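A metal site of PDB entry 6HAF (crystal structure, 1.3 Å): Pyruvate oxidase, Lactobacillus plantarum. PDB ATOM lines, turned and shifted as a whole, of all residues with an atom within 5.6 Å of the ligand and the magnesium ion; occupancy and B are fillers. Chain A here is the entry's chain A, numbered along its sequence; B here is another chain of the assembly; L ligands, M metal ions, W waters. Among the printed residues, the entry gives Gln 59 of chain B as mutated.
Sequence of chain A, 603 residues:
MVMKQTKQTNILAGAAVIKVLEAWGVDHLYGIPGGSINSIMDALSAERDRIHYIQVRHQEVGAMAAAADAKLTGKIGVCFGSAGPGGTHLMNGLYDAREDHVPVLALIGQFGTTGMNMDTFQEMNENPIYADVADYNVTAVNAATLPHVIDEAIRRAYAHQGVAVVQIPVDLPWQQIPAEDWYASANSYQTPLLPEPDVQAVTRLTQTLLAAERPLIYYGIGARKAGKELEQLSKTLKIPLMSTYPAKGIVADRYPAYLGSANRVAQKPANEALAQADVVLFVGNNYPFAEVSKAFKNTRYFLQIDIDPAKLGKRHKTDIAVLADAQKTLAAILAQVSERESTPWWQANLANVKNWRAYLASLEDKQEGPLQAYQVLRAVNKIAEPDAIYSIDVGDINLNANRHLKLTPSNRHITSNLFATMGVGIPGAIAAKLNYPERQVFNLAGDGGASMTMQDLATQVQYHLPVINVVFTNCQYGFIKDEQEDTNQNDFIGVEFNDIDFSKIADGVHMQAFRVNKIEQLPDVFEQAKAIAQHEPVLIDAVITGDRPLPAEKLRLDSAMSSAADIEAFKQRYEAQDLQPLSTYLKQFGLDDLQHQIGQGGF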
ATOM      1  N   ASN A  92     -20.097  15.933 -31.545  1.00  0.00           N
ATOM      2  CA  ASN A  92     -18.967  16.805 -31.186  1.00  0.00           C
ATOM      3  C   ASN A  92     -17.905  16.069 -30.373  1.00  0.00           C
ATOM      4  O   ASN A  92     -16.694  16.332 -30.529  1.00  0.00           O
ATOM      5  CB  ASN A  92     -19.400  18.080 -30.525  1.00  0.00           C
ATOM      6  CG  ASN A  92     -19.870  19.101 -31.532  1.00  0.00           C
ATOM      7  OD1 ASN A  92     -20.655  18.772 -32.422  1.00  0.00           O
ATOM      8  ND2 ASN A  92     -19.341  20.325 -31.447  1.00  0.00           N
ATOM      9  N   ASP A 393     -11.847  24.413 -21.396  1.00  0.00           N
ATOM     10  CA  ASP A 393     -12.757  24.588 -22.519  1.00  0.00           C
ATOM     11  C   ASP A 393     -11.991  25.312 -23.647  1.00  0.00           C
ATOM     12  O   ASP A 393     -10.747  25.251 -23.677  1.00  0.00           O
ATOM     13  CB  ASP A 393     -14.027  25.315 -22.051  1.00  0.00           C
ATOM     14  CG  ASP A 393     -15.261  24.894 -22.808  1.00  0.00           C
ATOM     15  OD1 ASP A 393     -15.424  25.333 -23.964  1.00  0.00           O
ATOM     16  OD2 ASP A 393     -16.091  24.155 -22.224  1.00  0.00           O
ATOM     17  N   VAL A 394     -12.721  25.953 -24.575  1.00  0.00           N
ATOM     18  CA  VAL A 394     -12.115  26.481 -25.800  1.00  0.00           C
ATOM     19  C   VAL A 394     -12.426  27.960 -25.937  1.00  0.00           C
ATOM     20  O   VAL A 394     -13.591  28.364 -25.931  1.00  0.00           O
ATOM     21  CB  VAL A 394     -12.642  25.708 -27.027  1.00  0.00           C
ATOM     22  CG1 VAL A 394     -12.238  26.342 -28.355  1.00  0.00           C
ATOM     23  CG2 VAL A 394     -12.139  24.259 -26.985  1.00  0.00           C
ATOM     24  N   GLY A 395     -11.377  28.742 -26.130  1.00  0.00           N
ATOM     25  CA  GLY A 395     -11.488  30.184 -26.275  1.00  0.00           C
ATOM     26  C   GLY A 395     -10.318  30.904 -25.638  1.00  0.00           C
ATOM     27  O   GLY A 395      -9.225  30.343 -25.549  1.00  0.00           O
ATOM     28  N   ASP A 396     -10.544  32.124 -25.150  1.00  0.00           N
ATOM     29  CA  ASP A 396      -9.452  32.841 -24.462  1.00  0.00           C
ATOM     30  C   ASP A 396      -8.854  32.017 -23.320  1.00  0.00           C
ATOM     31  O   ASP A 396      -7.694  32.196 -22.989  1.00  0.00           O
ATOM     32  CB  ASP A 396      -9.921  34.173 -23.867  1.00  0.00           C
ATOM     33  CG  ASP A 396      -9.996  35.327 -24.856  1.00  0.00           C
ATOM     34  OD1 ASP A 396      -9.440  35.244 -25.977  1.00  0.00           O
ATOM     35  OD2 ASP A 396     -10.648  36.347 -24.486  1.00  0.00           O
ATOM     36  N   ILE A 397      -9.623  31.112 -22.729  1.00  0.00           N
ATOM     37  CA  ILE A 397      -9.084  30.352 -21.617  1.00  0.00           C
ATOM     38  C   ILE A 397      -7.898  29.501 -22.034  1.00  0.00           C
ATOM     39  O   ILE A 397      -7.006  29.268 -21.228  1.00  0.00           O
ATOM     40  CB  ILE A 397     -10.155  29.474 -20.910  1.00  0.00           C
ATOM     41  CG1 ILE A 397      -9.620  28.842 -19.624  1.00  0.00           C
ATOM     42  CG2 ILE A 397     -10.732  28.359 -21.856  1.00  0.00           C
ATOM     43  CD1 ILE A 397      -9.147  29.779 -18.567  1.00  0.00           C
ATOM     44  N   PHE A 419      -9.901  19.450 -33.003  1.00  0.00           N
ATOM     45  CA  PHE A 419     -11.272  19.765 -33.381  1.00  0.00           C
ATOM     46  C   PHE A 419     -11.730  21.009 -32.649  1.00  0.00           C
ATOM     47  O   PHE A 419     -12.545  21.768 -33.146  1.00  0.00           O
ATOM     48  CB  PHE A 419     -12.168  18.570 -33.036  1.00  0.00           C
ATOM     49  CG  PHE A 419     -13.560  18.645 -33.590  1.00  0.00           C
ATOM     50  CD1 PHE A 419     -13.767  18.685 -34.965  1.00  0.00           C
ATOM     51  CD2 PHE A 419     -14.652  18.631 -32.762  1.00  0.00           C
ATOM     52  CE1 PHE A 419     -15.028  18.705 -35.487  1.00  0.00           C
ATOM     53  CE2 PHE A 419     -15.960  18.627 -33.294  1.00  0.00           C
ATOM     54  CZ  PHE A 419     -16.127  18.702 -34.655  1.00  0.00           C
ATOM     55  N   ALA A 420     -11.190  21.234 -31.456  1.00  0.00           N
ATOM     56  CA  ALA A 420     -11.441  22.440 -30.645  1.00  0.00           C
ATOM     57  C   ALA A 420     -12.920  22.713 -30.458  1.00  0.00           C
ATOM     58  O   ALA A 420     -13.386  23.833 -30.619  1.00  0.00           O
ATOM     59  CB  ALA A 420     -10.724  23.662 -31.232  1.00  0.00           C
ATOM     60  N   THR A 421     -13.651  21.687 -30.036  1.00  0.00           N
ATOM     61  CA  THR A 421     -15.041  21.896 -29.680  1.00  0.00           C
ATOM     62  C   THR A 421     -15.205  22.583 -28.318  1.00  0.00           C
ATOM     63  O   THR A 421     -14.770  22.103 -27.279  1.00  0.00           O
ATOM     64  CB  THR A 421     -15.911  20.613 -29.741  1.00  0.00           C
ATOM     65  OG1 THR A 421     -17.256  20.962 -29.431  1.00  0.00           O
ATOM     66  CG2 THR A 421     -15.427  19.525 -28.809  1.00  0.00           C
ATOM     67  N   MET A 422     -15.894  23.712 -28.319  1.00  0.00           N
ATOM     68  CA  MET A 422     -16.358  24.328 -27.092  1.00  0.00           C
ATOM     69  C   MET A 422     -17.256  23.328 -26.363  1.00  0.00           C
ATOM     70  O   MET A 422     -17.868  22.435 -26.972  1.00  0.00           O
ATOM     71  CB  MET A 422     -17.146  25.592 -27.401  1.00  0.00           C
ATOM     72  CG  MET A 422     -16.304  26.765 -27.843  1.00  0.00           C
ATOM     73  SD  MET A 422     -17.324  28.063 -28.555  1.00  0.00           S
ATOM     74  CE  MET A 422     -18.224  28.605 -27.131  1.00  0.00           C
ATOM     75  N   ALA A 445     -13.478  27.377 -17.896  1.00  0.00           N
ATOM     76  CA  ALA A 445     -14.307  27.550 -19.078  1.00  0.00           C
ATOM     77  C   ALA A 445     -14.715  29.006 -19.264  1.00  0.00           C
ATOM     78  O   ALA A 445     -15.054  29.676 -18.296  1.00  0.00           O
ATOM     79  CB  ALA A 445     -15.558  26.665 -18.999  1.00  0.00           C
ATOM     80  N   GLY A 446     -14.772  29.453 -20.515  1.00  0.00           N
ATOM     81  CA  GLY A 446     -15.426  30.704 -20.803  1.00  0.00           C
ATOM     82  C   GLY A 446     -16.928  30.572 -20.695  1.00  0.00           C
ATOM     83  O   GLY A 446     -17.471  29.471 -20.677  1.00  0.00           O
ATOM     84  N   ASP A 447     -17.612  31.712 -20.630  1.00  0.00           N
ATOM     85  CA  ASP A 447     -19.057  31.716 -20.527  1.00  0.00           C
ATOM     86  C   ASP A 447     -19.742  31.104 -21.748  1.00  0.00           C
ATOM     87  O   ASP A 447     -20.756  30.423 -21.615  1.00  0.00           O
ATOM     88  CB  ASP A 447     -19.627  33.095 -20.165  1.00  0.00           C
ATOM     89  CG  ASP A 447     -19.130  34.274 -21.025  1.00  0.00           C
ATOM     90  OD1 ASP A 447     -18.274  34.152 -21.946  1.00  0.00           O
ATOM     91  OD2 ASP A 447     -19.620  35.375 -20.694  1.00  0.00           O
ATOM     92  N   GLY A 448     -19.217  31.324 -22.945  1.00  0.00           N
ATOM     93  CA  GLY A 448     -19.801  30.754 -24.140  1.00  0.00           C
ATOM     94  C   GLY A 448     -19.716  29.235 -24.111  1.00  0.00           C
ATOM     95  O   GLY A 448     -20.700  28.529 -24.372  1.00  0.00           O
ATOM     96  N   GLY A 449     -18.561  28.718 -23.734  1.00  0.00           N
ATOM     97  CA  GLY A 449     -18.356  27.279 -23.696  1.00  0.00           C
ATOM     98  C   GLY A 449     -19.115  26.591 -22.575  1.00  0.00           C
ATOM     99  O   GLY A 449     -19.718  25.528 -22.751  1.00  0.00           O
ATOM    100  N   ALA A 450     -19.084  27.188 -21.392  1.00  0.00           N
ATOM    101  CA  ALA A 450     -19.807  26.668 -20.253  1.00  0.00           C
ATOM    102  C   ALA A 450     -21.289  26.658 -20.567  1.00  0.00           C
ATOM    103  O   ALA A 450     -22.002  25.712 -20.187  1.00  0.00           O
ATOM    104  CB  ALA A 450     -19.526  27.533 -19.015  1.00  0.00           C
ATOM    105  N   MET A 452     -22.737  26.119 -23.358  1.00  0.00           N
ATOM    106  CA  MET A 452     -23.104  25.057 -24.278  1.00  0.00           C
ATOM    107  C   MET A 452     -23.416  23.740 -23.584  1.00  0.00           C
ATOM    108  O   MET A 452     -24.220  22.966 -24.078  1.00  0.00           O
ATOM    109  CB  MET A 452     -22.038  24.850 -25.353  1.00  0.00           C
ATOM    110  CG  MET A 452     -22.088  25.961 -26.382  1.00  0.00           C
ATOM    111  SD  MET A 452     -20.824  25.727 -27.625  1.00  0.00           S
ATOM    112  CE  MET A 452     -21.161  27.117 -28.669  1.00  0.00           C
ATOM    113  N   PHE A 472     -15.414  32.033 -16.771  1.00  0.00           N
ATOM    114  CA  PHE A 472     -14.846  33.366 -17.071  1.00  0.00           C
ATOM    115  C   PHE A 472     -15.898  34.142 -17.869  1.00  0.00           C
ATOM    116  O   PHE A 472     -16.051  33.941 -19.065  1.00  0.00           O
ATOM    117  CB  PHE A 472     -13.542  33.182 -17.857  1.00  0.00           C
ATOM    118  CG  PHE A 472     -12.401  32.601 -17.054  1.00  0.00           C
ATOM    119  CD1 PHE A 472     -11.321  33.407 -16.694  1.00  0.00           C
ATOM    120  CD2 PHE A 472     -12.387  31.293 -16.657  1.00  0.00           C
ATOM    121  CE1 PHE A 472     -10.280  32.868 -15.954  1.00  0.00           C
ATOM    122  CE2 PHE A 472     -11.360  30.783 -15.926  1.00  0.00           C
ATOM    123  CZ  PHE A 472     -10.314  31.565 -15.573  1.00  0.00           C
ATOM    124  N   THR A 473     -16.648  34.986 -17.162  1.00  0.00           N
ATOM    125  CA  THR A 473     -17.805  35.664 -17.717  1.00  0.00           C
ATOM    126  C   THR A 473     -17.380  37.042 -18.202  1.00  0.00           C
ATOM    127  O   THR A 473     -17.212  37.961 -17.407  1.00  0.00           O
ATOM    128  CB  THR A 473     -18.972  35.685 -16.739  1.00  0.00           C
ATOM    129  OG1 THR A 473     -19.472  34.337 -16.614  1.00  0.00           O
ATOM    130  CG2 THR A 473     -20.101  36.593 -17.254  1.00  0.00           C
ATOM    131  N   ASN A 474     -17.170  37.149 -19.526  1.00  0.00           N
ATOM    132  CA  ASN A 474     -16.941  38.418 -20.179  1.00  0.00           C
ATOM    133  C   ASN A 474     -18.119  38.912 -21.001  1.00  0.00           C
ATOM    134  O   ASN A 474     -18.031  39.975 -21.572  1.00  0.00           O
ATOM    135  CB  ASN A 474     -15.657  38.397 -21.041  1.00  0.00           C
ATOM    136  CG  ASN A 474     -15.584  37.213 -21.984  1.00  0.00           C
ATOM    137  OD1 ASN A 474     -16.580  36.566 -22.259  1.00  0.00           O
ATOM    138  ND2 ASN A 474     -14.402  36.933 -22.486  1.00  0.00           N
ATOM    139  N   CYS A 475     -19.209  38.134 -21.047  1.00  0.00           N
ATOM    140  CA  CYS A 475     -20.368  38.439 -21.897  1.00  0.00           C
ATOM    141  C   CYS A 475     -19.958  38.574 -23.349  1.00  0.00           C
ATOM    142  O   CYS A 475     -20.540  39.367 -24.101  1.00  0.00           O
ATOM    143  CB  CYS A 475     -21.116  39.695 -21.429  1.00  0.00           C
ATOM    144  SG  CYS A 475     -21.832  39.487 -19.779  1.00  0.00           S
ATOM    145  N   GLN A 476     -18.987  37.763 -23.755  1.00  0.00           N
ATOM    146  CA  GLN A 476     -18.461  37.784 -25.109  1.00  0.00           C
ATOM    147  C   GLN A 476     -18.022  36.413 -25.558  1.00  0.00           C
ATOM    148  O   GLN A 476     -17.673  35.551 -24.747  1.00  0.00           O
ATOM    149  CB  GLN A 476     -17.224  38.676 -25.220  1.00  0.00           C
ATOM    150  CG  GLN A 476     -17.416  40.095 -24.851  1.00  0.00           C
ATOM    151  CD  GLN A 476     -16.097  40.862 -24.819  1.00  0.00           C
ATOM    152  OE1 GLN A 476     -15.024  40.281 -24.652  1.00  0.00           O
ATOM    153  NE2 GLN A 476     -16.172  42.154 -24.949  1.00  0.00           N
ATOM    154  N   TYR A 477     -17.985  36.226 -26.866  1.00  0.00           N
ATOM    155  CA  TYR A 477     -17.130  35.207 -27.455  1.00  0.00           C
ATOM    156  C   TYR A 477     -15.812  35.953 -27.697  1.00  0.00           C
ATOM    157  O   TYR A 477     -15.542  36.438 -28.808  1.00  0.00           O
ATOM    158  CB  TYR A 477     -17.699  34.684 -28.767  1.00  0.00           C
ATOM    159  CG  TYR A 477     -18.996  33.902 -28.630  1.00  0.00           C
ATOM    160  CD1 TYR A 477     -19.092  32.833 -27.748  1.00  0.00           C
ATOM    161  CD2 TYR A 477     -20.087  34.231 -29.380  1.00  0.00           C
ATOM    162  CE1 TYR A 477     -20.285  32.127 -27.626  1.00  0.00           C
ATOM    163  CE2 TYR A 477     -21.263  33.532 -29.269  1.00  0.00           C
ATOM    164  CZ  TYR A 477     -21.357  32.475 -28.394  1.00  0.00           C
ATOM    165  OH  TYR A 477     -22.538  31.813 -28.294  1.00  0.00           O
ATOM    166  N   GLY A 478     -15.024  36.115 -26.637  1.00  0.00           N
ATOM    167  CA  GLY A 478     -13.865  37.018 -26.704  1.00  0.00           C
ATOM    168  C   GLY A 478     -12.855  36.656 -27.776  1.00  0.00           C
ATOM    169  O   GLY A 478     -12.360  37.513 -28.544  1.00  0.00           O
ATOM    170  N   PHE A 479     -12.552  35.354 -27.850  1.00  0.00           N
ATOM    171  CA  PHE A 479     -11.579  34.871 -28.826  1.00  0.00           C
ATOM    172  C   PHE A 479     -11.979  35.289 -30.248  1.00  0.00           C
ATOM    173  O   PHE A 479     -11.127  35.606 -31.080  1.00  0.00           O
ATOM    174  CB  PHE A 479     -11.525  33.347 -28.708  1.00  0.00           C
ATOM    175  CG  PHE A 479     -10.223  32.708 -29.111  1.00  0.00           C
ATOM    176  CD1 PHE A 479      -9.085  32.881 -28.355  1.00  0.00           C
ATOM    177  CD2 PHE A 479     -10.177  31.868 -30.203  1.00  0.00           C
ATOM    178  CE1 PHE A 479      -7.914  32.255 -28.706  1.00  0.00           C
ATOM    179  CE2 PHE A 479      -9.000  31.224 -30.541  1.00  0.00           C
ATOM    180  CZ  PHE A 479      -7.857  31.420 -29.785  1.00  0.00           C
ATOM    181  N   ILE A 480     -13.281  35.249 -30.520  1.00  0.00           N
ATOM    182  CA  ILE A 480     -13.807  35.606 -31.846  1.00  0.00           C
ATOM    183  C   ILE A 480     -13.946  37.121 -32.029  1.00  0.00           C
ATOM    184  O   ILE A 480     -13.711  37.615 -33.144  1.00  0.00           O
ATOM    185  CB  ILE A 480     -15.169  34.941 -32.115  1.00  0.00           C
ATOM    186  CG1 ILE A 480     -15.082  33.454 -31.820  1.00  0.00           C
ATOM    187  CG2 ILE A 480     -15.628  35.190 -33.550  1.00  0.00           C
ATOM    188  CD1 ILE A 480     -13.943  32.702 -32.510  1.00  0.00           C
ATOM    189  N   PHE A 497     -22.849  39.581 -25.947  1.00  0.00           N
ATOM    190  CA  PHE A 497     -24.158  39.044 -25.647  1.00  0.00           C
ATOM    191  C   PHE A 497     -24.540  39.288 -24.193  1.00  0.00           C
ATOM    192  O   PHE A 497     -23.771  39.873 -23.432  1.00  0.00           O
ATOM    193  CB  PHE A 497     -24.254  37.560 -26.021  1.00  0.00           C
ATOM    194  CG  PHE A 497     -23.120  36.701 -25.534  1.00  0.00           C
ATOM    195  CD1 PHE A 497     -22.925  36.448 -24.180  1.00  0.00           C
ATOM    196  CD2 PHE A 497     -22.263  36.103 -26.449  1.00  0.00           C
ATOM    197  CE1 PHE A 497     -21.862  35.627 -23.757  1.00  0.00           C
ATOM    198  CE2 PHE A 497     -21.236  35.292 -26.031  1.00  0.00           C
ATOM    199  CZ  PHE A 497     -21.036  35.058 -24.699  1.00  0.00           C
ATOM    200  N   ILE B  32     -23.651  31.123 -34.698  1.00  0.00           N
ATOM    201  CA  ILE B  32     -22.613  31.557 -33.753  1.00  0.00           C
ATOM    202  C   ILE B  32     -21.399  31.803 -34.648  1.00  0.00           C
ATOM    203  O   ILE B  32     -21.062  30.964 -35.482  1.00  0.00           O
ATOM    204  CB  ILE B  32     -22.345  30.476 -32.694  1.00  0.00           C
ATOM    205  CG1 ILE B  32     -23.560  30.332 -31.776  1.00  0.00           C
ATOM    206  CG2 ILE B  32     -21.024  30.748 -31.923  1.00  0.00           C
ATOM    207  CD1 ILE B  32     -23.441  29.259 -30.763  1.00  0.00           C
ATOM    208  N   PRO B  33     -20.723  32.951 -34.478  1.00  0.00           N
ATOM    209  CA  PRO B  33     -19.571  33.279 -35.342  1.00  0.00           C
ATOM    210  C   PRO B  33     -18.343  32.491 -34.941  1.00  0.00           C
ATOM    211  O   PRO B  33     -18.253  31.860 -33.883  1.00  0.00           O
ATOM    212  CB  PRO B  33     -19.363  34.765 -35.057  1.00  0.00           C
ATOM    213  CG  PRO B  33     -19.734  34.882 -33.609  1.00  0.00           C
ATOM    214  CD  PRO B  33     -20.972  33.998 -33.468  1.00  0.00           C
ATOM    215  N   GLY B  34     -17.395  32.495 -35.862  1.00  0.00           N
ATOM    216  CA  GLY B  34     -16.055  31.951 -35.656  1.00  0.00           C
ATOM    217  C   GLY B  34     -15.177  32.503 -36.748  1.00  0.00           C
ATOM    218  O   GLY B  34     -15.665  33.006 -37.756  1.00  0.00           O
ATOM    219  N   GLN B  59     -25.402  25.942 -31.458  1.00  0.00           N
ATOM    220  CA  GLN B  59     -25.830  25.898 -32.845  1.00  0.00           C
ATOM    221  C   GLN B  59     -26.968  24.926 -33.136  1.00  0.00           C
ATOM    222  O   GLN B  59     -27.667  25.112 -34.147  1.00  0.00           O
ATOM    223  CB  GLN B  59     -24.658  25.595 -33.788  1.00  0.00           C
ATOM    224  CG  GLN B  59     -23.465  26.572 -33.710  1.00  0.00           C
ATOM    225  CD  GLN B  59     -22.435  26.219 -32.666  1.00  0.00           C
ATOM    226  OE1 GLN B  59     -22.704  25.450 -31.732  1.00  0.00           O
ATOM    227  NE2 GLN B  59     -21.297  26.860 -32.741  1.00  0.00           N
ATOM    228  N   SER B  82     -19.745  27.651 -37.605  1.00  0.00           N
ATOM    229  CA  SER B  82     -18.348  27.691 -37.949  1.00  0.00           C
ATOM    230  C   SER B  82     -17.758  26.281 -38.216  1.00  0.00           C
ATOM    231  O   SER B  82     -18.388  25.251 -37.954  1.00  0.00           O
ATOM    232  CB  SER B  82     -17.587  28.439 -36.834  1.00  0.00           C
ATOM    233  OG  SER B  82     -17.767  27.809 -35.553  1.00  0.00           O
ATOM    234  N   PRO B  85     -16.621  21.900 -35.189  1.00  0.00           N
ATOM    235  CA  PRO B  85     -17.651  21.758 -34.139  1.00  0.00           C
ATOM    236  C   PRO B  85     -18.845  22.692 -34.235  1.00  0.00           C
ATOM    237  O   PRO B  85     -19.936  22.360 -33.721  1.00  0.00           O
ATOM    238  CB  PRO B  85     -16.867  22.031 -32.848  1.00  0.00           C
ATOM    239  CG  PRO B  85     -15.722  22.921 -33.280  1.00  0.00           C
ATOM    240  CD  PRO B  85     -15.328  22.300 -34.606  1.00  0.00           C
ATOM    241  N   GLY B  86     -18.682  23.832 -34.902  1.00  0.00           N
ATOM    242  CA  GLY B  86     -19.819  24.712 -35.070  1.00  0.00           C
ATOM    243  C   GLY B  86     -20.883  24.077 -35.929  1.00  0.00           C
ATOM    244  O   GLY B  86     -22.066  24.094 -35.596  1.00  0.00           O
ATOM    245  N   HIS B  89     -22.484  20.712 -34.490  1.00  0.00           N
ATOM    246  CA  HIS B  89     -23.575  21.021 -33.576  1.00  0.00           C
ATOM    247  C   HIS B  89     -24.970  21.250 -34.220  1.00  0.00           C
ATOM    248  O   HIS B  89     -25.983  21.150 -33.546  1.00  0.00           O
ATOM    249  CB  HIS B  89     -23.241  22.241 -32.745  1.00  0.00           C
ATOM    250  CG  HIS B  89     -22.610  21.951 -31.406  1.00  0.00           C
ATOM    251  ND1 HIS B  89     -22.168  22.961 -30.577  1.00  0.00           N
ATOM    252  CD2 HIS B  89     -22.449  20.799 -30.691  1.00  0.00           C
ATOM    253  CE1 HIS B  89     -21.753  22.453 -29.432  1.00  0.00           C
ATOM    254  NE2 HIS B  89     -21.910  21.143 -29.473  1.00  0.00           N
ATOM    255  N   GLN B 122      -8.314  22.890 -36.819  1.00  0.00           N
ATOM    256  CA  GLN B 122      -9.758  22.660 -37.008  1.00  0.00           C
ATOM    257  C   GLN B 122     -10.150  22.584 -38.473  1.00  0.00           C
ATOM    258  O   GLN B 122     -11.263  22.880 -38.829  1.00  0.00           O
ATOM    259  CB  GLN B 122     -10.526  23.786 -36.339  1.00  0.00           C
ATOM    260  CG  GLN B 122     -12.008  23.520 -36.041  1.00  0.00           C
ATOM    261  CD  GLN B 122     -12.522  24.640 -35.252  1.00  0.00           C
ATOM    262  OE1 GLN B 122     -12.798  24.514 -34.065  1.00  0.00           O
ATOM    263  NE2 GLN B 122     -12.663  25.769 -35.900  1.00  0.00           N
HETATM  264  N1  LIG L   1     -18.708  26.482 -31.649  1.00  0.00           N
HETATM  265  C1  LIG L   1     -18.106  25.411 -31.088  1.00  0.00           C
HETATM  266  C2  LIG L   1     -18.985  24.287 -30.565  1.00  0.00           C
HETATM  267  N2  LIG L   1     -16.773  25.324 -30.983  1.00  0.00           N
HETATM  268  C3  LIG L   1     -16.023  26.332 -31.449  1.00  0.00           C
HETATM  269  N3  LIG L   1     -14.703  26.160 -31.369  1.00  0.00           N
HETATM  270  C4  LIG L   1     -16.620  27.478 -32.005  1.00  0.00           C
HETATM  271  C5  LIG L   1     -18.007  27.512 -32.070  1.00  0.00           C
HETATM  272  C6  LIG L   1     -15.811  28.686 -32.523  1.00  0.00           C
HETATM  273  N4  LIG L   1     -15.210  29.412 -31.380  1.00  0.00           N
HETATM  274  C7  LIG L   1     -13.930  29.174 -31.000  1.00  0.00           C
HETATM  275  S1  LIG L   1     -13.505  30.171 -29.622  1.00  0.00           S
HETATM  276  C8  LIG L   1     -15.123  30.803 -29.551  1.00  0.00           C
HETATM  277  C9  LIG L   1     -15.890  30.299 -30.608  1.00  0.00           C
HETATM  278  C10 LIG L   1     -17.347  30.673 -30.853  1.00  0.00           C
HETATM  279  C11 LIG L   1     -15.471  31.769 -28.460  1.00  0.00           C
HETATM  280  C12 LIG L   1     -15.479  31.085 -27.078  1.00  0.00           C
HETATM  281  O1  LIG L   1     -16.185  32.005 -26.237  1.00  0.00           O
HETATM  282  P1  LIG L   1     -16.110  31.812 -24.653  1.00  0.00           P
HETATM  283  O2  LIG L   1     -17.034  32.808 -24.047  1.00  0.00           O
HETATM  284  O3  LIG L   1     -16.326  30.374 -24.291  1.00  0.00           O
HETATM  285  O4  LIG L   1     -14.592  32.198 -24.310  1.00  0.00           O
HETATM  286  P2  LIG L   1     -13.864  33.658 -24.284  1.00  0.00           P
HETATM  287  O5  LIG L   1     -14.937  34.723 -24.293  1.00  0.00           O
HETATM  288  O6  LIG L   1     -12.933  33.693 -25.537  1.00  0.00           O
HETATM  289  O7  LIG L   1     -13.090  33.611 -22.929  1.00  0.00           O
HETATM  290 MG    MG M   1     -16.752  34.608 -23.175  1.00  0.00          MG
HETATM  291  O   HOH W   1     -15.626  26.431 -35.155  1.00  0.00           O
HETATM  292  O   HOH W   2     -15.463  33.941 -21.639  1.00  0.00           O
HETATM  293  O   HOH W   3     -14.407  28.825 -23.247  1.00  0.00           O
HETATM  294  O   HOH W   4     -12.313  27.160 -32.834  1.00  0.00           O
HETATM  295  O   HOH W   5     -12.459  30.918 -22.627  1.00  0.00           O
HETATM  296  O   HOH W   6     -10.693  28.782 -31.697  1.00  0.00           O
HETATM  297  O   HOH W   7     -11.783  34.655 -20.815  1.00  0.00           O
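NE2 of Gln 59 of chain B sits at hydrogen-bond distance from N1 of the ligand, 2.8 Å away. N3 of the ligand sits at hydrogen-bond distance from O of Ala 420, at 2.8 Å. An oxygen (O3) of the ligand sits at hydrogen-bond distance from the backbone NH (N) of Gly 448. An oxygen (O6) of the ligand sits at hydrogen-bond distance from the backbone NH (N) of Gly 478 (3.4 Å). The backbone NH (N) of Gly 449 is in hydrogen-bond range of an oxygen (O3) of the ligand (2.8 Å). O6 of the ligand lies within hydrogen-bond range of N of Phe 479. The backbone NH (N) of Asp 396 sits at hydrogen-bond distance from an oxygen (O6) of the ligand. The backbone NH (N) of Met 422 is in hydrogen-bond range of a nitrogen (N2) of the ligand (3.2 Å).
The backbone carbonyl oxygen of Phe 472 sits at hydrogen-bond distance from the backbone NH of Asp 447 (3.1 Å). A ring nitrogen (ND1) of His 89 of chain B is in hydrogen-bond range of the side-chain amide oxygen (OE1) of Gln 59 of chain B (2.8 Å). OG1 of Thr 421 lies within hydrogen-bond range of ND2 of Asn 92 (3.0 Å). The side-chain amide nitrogen (ND2) of Asn 92 lies within hydrogen-bond range of the backbone carbonyl oxygen (O) of Pro 85 of chain B (3.1 Å). OE1 of Gln 122 of chain B lies close to O of Phe 419 (2.9 Å). A ring nitrogen (NE2) of His 89 of chain B lies close to the side-chain amide nitrogen (ND2) of Asn 92, at 3.3 Å. The side-chain carboxylate of Asp 447 lies within hydrogen-bond range of the backbone NH of Cys 475.
O of Val 394 touches C12 of the ligand (3.5 Å). Gly 395 touches the ligand. Thr 421 touches the ligand. CA of Gly 446 touches O3 of the ligand, 3.6 Å away. SD of Met 452 touches C2 of the ligand, at 3.8 Å. Tyr 477 touches the ligand. CG1 of Ile 480 touches C9 of the ligand (3.5 Å). Ile 32 of chain B touches the ligand. Pro 33 of chain B touches the ligand (O to C10, 3.4 Å). Ser 82 of chain B touches the ligand (OG to C5, 3.5 Å). CG of Pro 85 of chain B touches N2 of the ligand, at 3.5 Å. His 89 of chain B touches the ligand. OE1 of Gln 122 of chain B touches N3 of the ligand, 3.7 Å away. Hydrophobic or aromatic side chains that line the ligand: Val 394, Met 422, Met 452, Tyr 477, Phe 479, Ile 480, Ile 32 of chain B, Pro 85 of chain B and His 89 of chain B. The nearest printed residue that does not touch the ligand is Gly 86 of chain B (4.01 Å).
Of the 36 residues printed, 3 come within 4 Å of the magnesium ion. Along chain A the residues within 4 Å of the magnesium ion span positions 447 to 476. The nearest printed residue that does not touch the magnesium ion is Gly 448 (4.1 Å).
The magnesium ion is bound by OD1 of Asp 447 (2.0 Å), O2 of the ligand (2.0 Å), O of Gln 476 (2.1 Å), water W2 (2.1 Å), O5 of the ligand (2.1 Å) and OD1 of Asn 474 (2.2 Å).
Water W2 lies within hydrogen-bond range of O of Phe 472 (2.6 Å), O7 of the ligand (2.7 Å), N of Asp 447 (3.3 Å) and ND2 of Asn 474 (3.3 Å). Water W3 lies within hydrogen-bond range of an oxygen (O3) of the ligand (2.7 Å), the backbone NH (N) of Gly 446 (2.8 Å) and the backbone carbonyl oxygen (O) of Val 394 (2.8 Å). Water W4 lies within hydrogen-bond range of OE1 of Gln 122 of chain B (3.0 Å) and N3 of the ligand (3.0 Å). Water W1 bridges the side-chain hydroxyl (OG) of Ser 82 of chain B (2.6 Å) and the side-chain amide nitrogen (NE2) of Gln 122 of chain B (3.1 Å).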
